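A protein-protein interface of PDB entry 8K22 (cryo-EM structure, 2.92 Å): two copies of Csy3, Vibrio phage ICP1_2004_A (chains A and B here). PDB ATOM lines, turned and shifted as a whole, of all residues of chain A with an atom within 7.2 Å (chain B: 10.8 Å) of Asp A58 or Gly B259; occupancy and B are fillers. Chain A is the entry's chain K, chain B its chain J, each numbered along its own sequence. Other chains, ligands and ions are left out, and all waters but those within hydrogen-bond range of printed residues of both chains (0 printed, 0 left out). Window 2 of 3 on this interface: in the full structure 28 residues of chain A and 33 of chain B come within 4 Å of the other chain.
No position is printed for both chains.
The side-chain amide nitrogen of Asn A53 lies close to the side-chain amide nitrogen of Asn A55, 3.4 Å away.
ND2 of Asn A53 lies within hydrogen-bond range of OD2 of Asp A56.
OE1 of Gln A48 sits close to OD1 of Asn A53, 3.3 Å away.
The backbone NH (N) of Ala B264 is in hydrogen-bond range of the backbone carbonyl oxygen (O) of Tyr B252 (3.4 Å).
The side-chain carboxylate of Asp A56 is in salt-bridge range of the side-chain amino group of Lys A59 (3.6 Å).
The side-chain amide nitrogen (NE2) of Gln A48 sits at hydrogen-bond distance from the backbone carbonyl oxygen (O) of Gly A60, at 2.5 Å.
Printed residues of chain B within 4 Å of Pro A54: Tyr B252 (3.4 Å) and Ala B264 (3.9 Å).
Of chain B, only Val B256, Gly B259 and Val B260 come within 4 Å of Asp A58.
Of chain B, only Val B256 (3.7 Å) comes within 4 Å of Lys A59.
Gly A60 touches one residue of chain B.
Pro B251 touches none of the printed residues of chain A.
Gly B253 touches none of the printed residues of chain A.
Printed residues of chain A within 4 Å of Ser B254: Thr A47 (3.2 Å) and Ala A57 (3.6 Å).
Of the printed residues of chain A, Val B260 touches Asp A58.
Of the printed residues of chain A, Ala B261 touches Ala A57.
Of the printed residues of chain A, Ala B264 touches Pro A54 (3.9 Å).
Printed residues of chain B that touch a printed residue of chain A: Glu B250, Tyr B252, Ser B254, Val B256, Gly B259, Val B260, Ala B261 and Ala B264.
Of the 11 printed residues of chain A, 7 touch a printed residue of chain B.
Printed residues of chain A that touch a printed residue of chain B: Thr A47, Asn A53, Pro A54, Ala A57, Asp A58, Lys A59 and Gly A60.
Among the printed residues, 14 pairs touch across the chains.
The side-chain hydroxyl (OH) of Tyr B252 lies close to the backbone nitrogen (N) of Pro A54, at 3.4 Å.
OG of Ser B254 lies within hydrogen-bond range of OG1 of Thr A47, at 3.2 Å.
OH of Tyr B252 sits at hydrogen-bond distance from N of Asn A53, 3.0 Å away.
OG1 of Thr A47 touches CG of Glu B250, 3.3 Å away.
Val B256 touches Thr A47 (CG1 to CG2, 3.7 Å).
O of Pro A54 touches CB of Ala B264, 3.9 Å away.
Tyr B252 touches Ala A57 (CG to CB, 3.6 Å).
Ser B254 touches Ala A57 (CB to O, 3.6 Å).
Ala A57 touches Ala B261 (CB to CB, 3.9 Å).
CG1 of Val B256 touches O of Asp A58, 3.7 Å away.
Asp A58 touches Gly B259 (CB to O, 3.4 Å).
Asp A58 touches Val B260 (CA to O, 3.6 Å).
Val B256 touches Gly A60.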
ATOM      1  N   GLY A  46     -10.106 -30.208  11.829  1.00  0.00           N
ATOM      2  CA  GLY A  46     -10.250 -30.201  13.266  1.00  0.00           C
ATOM      3  C   GLY A  46      -8.943 -29.803  13.908  1.00  0.00           C
ATOM      4  O   GLY A  46      -8.043 -29.309  13.226  1.00  0.00           O
ATOM      5  N   THR A  47      -8.820 -30.007  15.211  1.00  0.00           N
ATOM      6  CA  THR A  47      -7.591 -29.708  15.928  1.00  0.00           C
ATOM      7  C   THR A  47      -6.945 -31.013  16.362  1.00  0.00           C
ATOM      8  O   THR A  47      -7.623 -31.895  16.898  1.00  0.00           O
ATOM      9  CB  THR A  47      -7.862 -28.832  17.148  1.00  0.00           C
ATOM     10  OG1 THR A  47      -8.155 -29.671  18.270  1.00  0.00           O
ATOM     11  CG2 THR A  47      -9.044 -27.913  16.890  1.00  0.00           C
ATOM     12  N   GLN A  48      -5.641 -31.138  16.129  1.00  0.00           N
ATOM     13  CA  GLN A  48      -4.933 -32.335  16.558  1.00  0.00           C
ATOM     14  C   GLN A  48      -4.728 -32.289  18.067  1.00  0.00           C
ATOM     15  O   GLN A  48      -4.074 -31.381  18.588  1.00  0.00           O
ATOM     16  CB  GLN A  48      -3.603 -32.465  15.826  1.00  0.00           C
ATOM     17  CG  GLN A  48      -2.928 -31.156  15.522  1.00  0.00           C
ATOM     18  CD  GLN A  48      -1.677 -31.336  14.699  1.00  0.00           C
ATOM     19  OE1 GLN A  48      -0.617 -31.660  15.225  1.00  0.00           O
ATOM     20  NE2 GLN A  48      -1.790 -31.114  13.399  1.00  0.00           N
ATOM     21  N   ASN A  53       0.736 -33.899  22.559  1.00  0.00           N
ATOM     22  CA  ASN A  53       0.862 -32.856  21.535  1.00  0.00           C
ATOM     23  C   ASN A  53       0.448 -31.438  21.941  1.00  0.00           C
ATOM     24  O   ASN A  53      -0.351 -30.821  21.244  1.00  0.00           O
ATOM     25  CB  ASN A  53       0.047 -33.244  20.303  1.00  0.00           C
ATOM     26  CG  ASN A  53       0.883 -33.300  19.046  1.00  0.00           C
ATOM     27  OD1 ASN A  53       0.354 -33.334  17.935  1.00  0.00           O
ATOM     28  ND2 ASN A  53       2.199 -33.308  19.212  1.00  0.00           N
ATOM     29  N   PRO A  54       0.993 -30.896  23.051  1.00  0.00           N
ATOM     30  CA  PRO A  54       0.576 -29.519  23.346  1.00  0.00           C
ATOM     31  C   PRO A  54       1.279 -28.530  22.438  1.00  0.00           C
ATOM     32  O   PRO A  54       0.745 -27.454  22.177  1.00  0.00           O
ATOM     33  CB  PRO A  54       1.035 -29.312  24.798  1.00  0.00           C
ATOM     34  CG  PRO A  54       1.429 -30.662  25.305  1.00  0.00           C
ATOM     35  CD  PRO A  54       1.891 -31.411  24.099  1.00  0.00           C
ATOM     36  N   ASN A  55       2.461 -28.891  21.953  1.00  0.00           N
ATOM     37  CA  ASN A  55       3.223 -28.022  21.070  1.00  0.00           C
ATOM     38  C   ASN A  55       2.552 -27.883  19.719  1.00  0.00           C
ATOM     39  O   ASN A  55       2.703 -26.864  19.050  1.00  0.00           O
ATOM     40  CB  ASN A  55       4.616 -28.614  20.876  1.00  0.00           C
ATOM     41  CG  ASN A  55       4.677 -30.085  21.246  1.00  0.00           C
ATOM     42  OD1 ASN A  55       4.956 -30.437  22.392  1.00  0.00           O
ATOM     43  ND2 ASN A  55       4.415 -30.953  20.275  1.00  0.00           N
ATOM     44  N   ASP A  56       1.822 -28.911  19.303  1.00  0.00           N
ATOM     45  CA  ASP A  56       1.182 -28.879  17.999  1.00  0.00           C
ATOM     46  C   ASP A  56      -0.327 -28.784  18.112  1.00  0.00           C
ATOM     47  O   ASP A  56      -1.038 -29.001  17.143  1.00  0.00           O
ATOM     48  CB  ASP A  56       1.569 -30.114  17.195  1.00  0.00           C
ATOM     49  CG  ASP A  56       3.064 -30.253  17.032  1.00  0.00           C
ATOM     50  OD1 ASP A  56       3.724 -29.244  16.712  1.00  0.00           O
ATOM     51  OD2 ASP A  56       3.580 -31.372  17.230  1.00  0.00           O
ATOM     52  N   ALA A  57      -0.823 -28.451  19.295  1.00  0.00           N
ATOM     53  CA  ALA A  57      -2.259 -28.289  19.475  1.00  0.00           C
ATOM     54  C   ALA A  57      -2.743 -27.106  18.671  1.00  0.00           C
ATOM     55  O   ALA A  57      -3.806 -27.162  18.055  1.00  0.00           O
ATOM     56  CB  ALA A  57      -2.558 -28.063  20.937  1.00  0.00           C
ATOM     57  N   ASP A  58      -1.968 -26.031  18.681  1.00  0.00           N
ATOM     58  CA  ASP A  58      -2.335 -24.819  17.963  1.00  0.00           C
ATOM     59  C   ASP A  58      -2.678 -25.016  16.491  1.00  0.00           C
ATOM     60  O   ASP A  58      -3.621 -24.397  15.997  1.00  0.00           O
ATOM     61  CB  ASP A  58      -1.175 -23.840  18.072  1.00  0.00           C
ATOM     62  CG  ASP A  58       0.138 -24.537  18.350  1.00  0.00           C
ATOM     63  OD1 ASP A  58       0.719 -25.104  17.402  1.00  0.00           O
ATOM     64  OD2 ASP A  58       0.581 -24.529  19.518  1.00  0.00           O
ATOM     65  N   LYS A  59      -1.926 -25.861  15.785  1.00  0.00           N
ATOM     66  CA  LYS A  59      -2.152 -26.028  14.360  1.00  0.00           C
ATOM     67  C   LYS A  59      -3.322 -26.973  14.106  1.00  0.00           C
ATOM     68  O   LYS A  59      -3.788 -27.688  14.994  1.00  0.00           O
ATOM     69  CB  LYS A  59      -0.888 -26.539  13.671  1.00  0.00           C
ATOM     70  CG  LYS A  59      -0.453 -27.920  14.112  1.00  0.00           C
ATOM     71  CD  LYS A  59       1.028 -28.152  13.844  1.00  0.00           C
ATOM     72  CE  LYS A  59       1.889 -27.030  14.403  1.00  0.00           C
ATOM     73  NZ  LYS A  59       3.282 -27.094  13.883  1.00  0.00           N
ATOM     74  N   GLY A  60      -3.793 -26.971  12.864  1.00  0.00           N
ATOM     75  CA  GLY A  60      -4.961 -27.732  12.483  1.00  0.00           C
ATOM     76  C   GLY A  60      -4.647 -29.190  12.221  1.00  0.00           C
ATOM     77  O   GLY A  60      -3.541 -29.682  12.448  1.00  0.00           O
ATOM     78  N   ILE B 247     -15.133 -20.682  23.856  1.00  0.00           N
ATOM     79  CA  ILE B 247     -14.504 -21.414  22.772  1.00  0.00           C
ATOM     80  C   ILE B 247     -15.070 -22.824  22.772  1.00  0.00           C
ATOM     81  O   ILE B 247     -15.741 -23.246  23.712  1.00  0.00           O
ATOM     82  CB  ILE B 247     -12.971 -21.438  22.885  1.00  0.00           C
ATOM     83  CG1 ILE B 247     -12.543 -22.317  24.054  1.00  0.00           C
ATOM     84  CG2 ILE B 247     -12.428 -20.032  23.037  1.00  0.00           C
ATOM     85  CD1 ILE B 247     -11.066 -22.520  24.144  1.00  0.00           C
ATOM     86  N   GLU B 250     -12.184 -28.569  23.072  1.00  0.00           N
ATOM     87  CA  GLU B 250     -11.170 -29.513  22.633  1.00  0.00           C
ATOM     88  C   GLU B 250     -10.462 -30.053  23.864  1.00  0.00           C
ATOM     89  O   GLU B 250     -10.605 -29.500  24.960  1.00  0.00           O
ATOM     90  CB  GLU B 250     -10.121 -28.914  21.667  1.00  0.00           C
ATOM     91  CG  GLU B 250     -10.490 -28.480  20.223  1.00  0.00           C
ATOM     92  CD  GLU B 250     -11.638 -27.510  20.011  1.00  0.00           C
ATOM     93  OE1 GLU B 250     -12.202 -26.974  20.966  1.00  0.00           O
ATOM     94  OE2 GLU B 250     -11.987 -27.285  18.835  1.00  0.00           O
ATOM     95  N   PRO B 251      -9.736 -31.169  23.731  1.00  0.00           N
ATOM     96  CA  PRO B 251      -8.811 -31.571  24.803  1.00  0.00           C
ATOM     97  C   PRO B 251      -7.734 -30.547  25.138  1.00  0.00           C
ATOM     98  O   PRO B 251      -7.277 -30.508  26.287  1.00  0.00           O
ATOM     99  CB  PRO B 251      -8.202 -32.868  24.256  1.00  0.00           C
ATOM    100  CG  PRO B 251      -9.285 -33.437  23.423  1.00  0.00           C
ATOM    101  CD  PRO B 251      -9.957 -32.274  22.776  1.00  0.00           C
ATOM    102  N   TYR B 252      -7.318 -29.716  24.188  1.00  0.00           N
ATOM    103  CA  TYR B 252      -6.284 -28.725  24.431  1.00  0.00           C
ATOM    104  C   TYR B 252      -6.821 -27.306  24.503  1.00  0.00           C
ATOM    105  O   TYR B 252      -6.024 -26.371  24.626  1.00  0.00           O
ATOM    106  CB  TYR B 252      -5.219 -28.811  23.339  1.00  0.00           C
ATOM    107  CG  TYR B 252      -4.209 -29.894  23.593  1.00  0.00           C
ATOM    108  CD1 TYR B 252      -3.448 -29.903  24.750  1.00  0.00           C
ATOM    109  CD2 TYR B 252      -4.042 -30.925  22.690  1.00  0.00           C
ATOM    110  CE1 TYR B 252      -2.533 -30.901  24.992  1.00  0.00           C
ATOM    111  CE2 TYR B 252      -3.136 -31.917  22.917  1.00  0.00           C
ATOM    112  CZ  TYR B 252      -2.381 -31.903  24.065  1.00  0.00           C
ATOM    113  OH  TYR B 252      -1.485 -32.918  24.278  1.00  0.00           O
ATOM    114  N   GLY B 253      -8.137 -27.124  24.423  1.00  0.00           N
ATOM    115  CA  GLY B 253      -8.728 -25.795  24.363  1.00  0.00           C
ATOM    116  C   GLY B 253      -8.281 -25.008  23.153  1.00  0.00           C
ATOM    117  O   GLY B 253      -8.124 -23.784  23.229  1.00  0.00           O
ATOM    118  N   SER B 254      -8.059 -25.687  22.035  1.00  0.00           N
ATOM    119  CA  SER B 254      -7.346 -25.118  20.904  1.00  0.00           C
ATOM    120  C   SER B 254      -8.330 -24.779  19.799  1.00  0.00           C
ATOM    121  O   SER B 254      -9.072 -25.648  19.335  1.00  0.00           O
ATOM    122  CB  SER B 254      -6.289 -26.088  20.384  1.00  0.00           C
ATOM    123  OG  SER B 254      -6.880 -27.317  20.011  1.00  0.00           O
ATOM    124  N   VAL B 255      -8.325 -23.521  19.378  1.00  0.00           N
ATOM    125  CA  VAL B 255      -8.977 -23.101  18.148  1.00  0.00           C
ATOM    126  C   VAL B 255      -7.875 -22.818  17.134  1.00  0.00           C
ATOM    127  O   VAL B 255      -6.769 -22.400  17.502  1.00  0.00           O
ATOM    128  CB  VAL B 255      -9.917 -21.905  18.379  1.00  0.00           C
ATOM    129  CG1 VAL B 255     -10.834 -22.199  19.547  1.00  0.00           C
ATOM    130  CG2 VAL B 255      -9.150 -20.657  18.707  1.00  0.00           C
ATOM    131  N   VAL B 256      -8.138 -23.136  15.866  1.00  0.00           N
ATOM    132  CA  VAL B 256      -7.065 -23.139  14.876  1.00  0.00           C
ATOM    133  C   VAL B 256      -7.055 -21.908  13.989  1.00  0.00           C
ATOM    134  O   VAL B 256      -6.077 -21.701  13.254  1.00  0.00           O
ATOM    135  CB  VAL B 256      -7.132 -24.400  13.997  1.00  0.00           C
ATOM    136  CG1 VAL B 256      -6.918 -25.628  14.848  1.00  0.00           C
ATOM    137  CG2 VAL B 256      -8.465 -24.472  13.279  1.00  0.00           C
ATOM    138  N   ARG B 257      -8.108 -21.090  14.015  1.00  0.00           N
ATOM    139  CA  ARG B 257      -8.053 -19.819  13.303  1.00  0.00           C
ATOM    140  C   ARG B 257      -7.076 -18.859  13.964  1.00  0.00           C
ATOM    141  O   ARG B 257      -6.205 -18.294  13.296  1.00  0.00           O
ATOM    142  CB  ARG B 257      -9.443 -19.202  13.206  1.00  0.00           C
ATOM    143  CG  ARG B 257     -10.535 -20.213  13.005  1.00  0.00           C
ATOM    144  CD  ARG B 257     -11.890 -19.643  13.371  1.00  0.00           C
ATOM    145  NE  ARG B 257     -12.576 -18.999  12.253  1.00  0.00           N
ATOM    146  CZ  ARG B 257     -13.106 -19.603  11.195  1.00  0.00           C
ATOM    147  NH1 ARG B 257     -13.038 -20.913  11.028  1.00  0.00           N
ATOM    148  NH2 ARG B 257     -13.722 -18.869  10.272  1.00  0.00           N
ATOM    149  N   ASN B 258      -7.165 -18.696  15.280  1.00  0.00           N
ATOM    150  CA  ASN B 258      -6.210 -17.823  15.947  1.00  0.00           C
ATOM    151  C   ASN B 258      -4.821 -18.437  16.072  1.00  0.00           C
ATOM    152  O   ASN B 258      -3.876 -17.711  16.399  1.00  0.00           O
ATOM    153  CB  ASN B 258      -6.738 -17.406  17.321  1.00  0.00           C
ATOM    154  CG  ASN B 258      -8.190 -16.970  17.276  1.00  0.00           C
ATOM    155  OD1 ASN B 258      -9.034 -17.493  17.993  1.00  0.00           O
ATOM    156  ND2 ASN B 258      -8.483 -16.003  16.417  1.00  0.00           N
ATOM    157  N   GLY B 259      -4.661 -19.726  15.780  1.00  0.00           N
ATOM    158  CA  GLY B 259      -3.349 -20.339  15.812  1.00  0.00           C
ATOM    159  C   GLY B 259      -2.794 -20.519  17.199  1.00  0.00           C
ATOM    160  O   GLY B 259      -1.575 -20.547  17.376  1.00  0.00           O
ATOM    161  N   VAL B 260      -3.667 -20.596  18.198  1.00  0.00           N
ATOM    162  CA  VAL B 260      -3.302 -20.682  19.602  1.00  0.00           C
ATOM    163  C   VAL B 260      -3.917 -21.933  20.215  1.00  0.00           C
ATOM    164  O   VAL B 260      -4.727 -22.629  19.599  1.00  0.00           O
ATOM    165  CB  VAL B 260      -3.743 -19.433  20.391  1.00  0.00           C
ATOM    166  CG1 VAL B 260      -3.432 -18.159  19.640  1.00  0.00           C
ATOM    167  CG2 VAL B 260      -5.229 -19.492  20.563  1.00  0.00           C
ATOM    168  N   ALA B 261      -3.504 -22.217  21.447  1.00  0.00           N
ATOM    169  CA  ALA B 261      -4.128 -23.230  22.289  1.00  0.00           C
ATOM    170  C   ALA B 261      -4.338 -22.622  23.669  1.00  0.00           C
ATOM    171  O   ALA B 261      -3.377 -22.423  24.420  1.00  0.00           O
ATOM    172  CB  ALA B 261      -3.274 -24.492  22.357  1.00  0.00           C
ATOM    173  N   TYR B 262      -5.594 -22.325  23.998  1.00  0.00           N
ATOM    174  CA  TYR B 262      -5.972 -21.690  25.255  1.00  0.00           C
ATOM    175  C   TYR B 262      -5.808 -22.563  26.491  1.00  0.00           C
ATOM    176  O   TYR B 262      -5.910 -22.035  27.603  1.00  0.00           O
ATOM    177  CB  TYR B 262      -7.419 -21.201  25.164  1.00  0.00           C
ATOM    178  CG  TYR B 262      -7.632 -19.969  24.314  1.00  0.00           C
ATOM    179  CD1 TYR B 262      -6.585 -19.109  24.027  1.00  0.00           C
ATOM    180  CD2 TYR B 262      -8.871 -19.694  23.758  1.00  0.00           C
ATOM    181  CE1 TYR B 262      -6.785 -17.971  23.275  1.00  0.00           C
ATOM    182  CE2 TYR B 262      -9.075 -18.571  22.982  1.00  0.00           C
ATOM    183  CZ  TYR B 262      -8.023 -17.720  22.736  1.00  0.00           C
ATOM    184  OH  TYR B 262      -8.211 -16.599  21.961  1.00  0.00           O
ATOM    185  N   ARG B 263      -5.565 -23.861  26.354  1.00  0.00           N
ATOM    186  CA  ARG B 263      -5.425 -24.706  27.529  1.00  0.00           C
ATOM    187  C   ARG B 263      -4.167 -25.562  27.520  1.00  0.00           C
ATOM    188  O   ARG B 263      -3.947 -26.318  28.472  1.00  0.00           O
ATOM    189  CB  ARG B 263      -6.666 -25.591  27.687  1.00  0.00           C
ATOM    190  CG  ARG B 263      -7.822 -24.880  28.345  1.00  0.00           C
ATOM    191  CD  ARG B 263      -9.085 -25.687  28.206  1.00  0.00           C
ATOM    192  NE  ARG B 263     -10.106 -25.324  29.180  1.00  0.00           N
ATOM    193  CZ  ARG B 263     -10.137 -25.751  30.434  1.00  0.00           C
ATOM    194  NH1 ARG B 263      -9.212 -26.567  30.909  1.00  0.00           N
ATOM    195  NH2 ARG B 263     -11.126 -25.356  31.230  1.00  0.00           N
ATOM    196  N   ALA B 264      -3.326 -25.453  26.498  1.00  0.00           N
ATOM    197  CA  ALA B 264      -2.079 -26.198  26.439  1.00  0.00           C
ATOM    198  C   ALA B 264      -0.928 -25.365  26.988  1.00  0.00           C
ATOM    199  O   ALA B 264      -0.897 -24.140  26.841  1.00  0.00           O
ATOM    200  CB  ALA B 264      -1.765 -26.631  25.007  1.00  0.00           C
ATOM    201  N   GLY B 265       0.021 -26.046  27.625  1.00  0.00           N
ATOM    202  CA  GLY B 265       1.200 -25.405  28.164  1.00  0.00           C
ATOM    203  C   GLY B 265       1.034 -24.790  29.533  1.00  0.00           C
ATOM    204  O   GLY B 265       2.002 -24.226  30.061  1.00  0.00           O
ATOM    205  N   ASN B 266      -0.155 -24.872  30.131  1.00  0.00           N
ATOM    206  CA  ASN B 266      -0.369 -24.308  31.458  1.00  0.00           C
ATOM    207  C   ASN B 266      -1.234 -25.189  32.361  1.00  0.00           C
ATOM    208  O   ASN B 266      -1.954 -24.661  33.218  1.00  0.00           O
ATOM    209  CB  ASN B 266      -0.853 -22.830  31.307  1.00  0.00           C
ATOM    210  CG  ASN B 266      -2.297 -22.667  30.791  1.00  0.00           C
ATOM    211  OD1 ASN B 266      -3.114 -23.574  30.785  1.00  0.00           O
ATOM    212  ND2 ASN B 266      -2.596 -21.453  30.344  1.00  0.00           N
ATOM    213  N   ASP B 269      -5.027 -28.419  30.223  1.00  0.00           N
ATOM    214  CA  ASP B 269      -5.505 -29.274  29.153  1.00  0.00           C
ATOM    215  C   ASP B 269      -6.117 -30.543  29.737  1.00  0.00           C
ATOM    216  O   ASP B 269      -5.845 -30.915  30.881  1.00  0.00           O
ATOM    217  CB  ASP B 269      -4.380 -29.574  28.154  1.00  0.00           C
ATOM    218  CG  ASP B 269      -3.103 -30.122  28.800  1.00  0.00           C
ATOM    219  OD1 ASP B 269      -3.124 -30.696  29.904  1.00  0.00           O
ATOM    220  OD2 ASP B 269      -2.035 -29.956  28.175  1.00  0.00           O
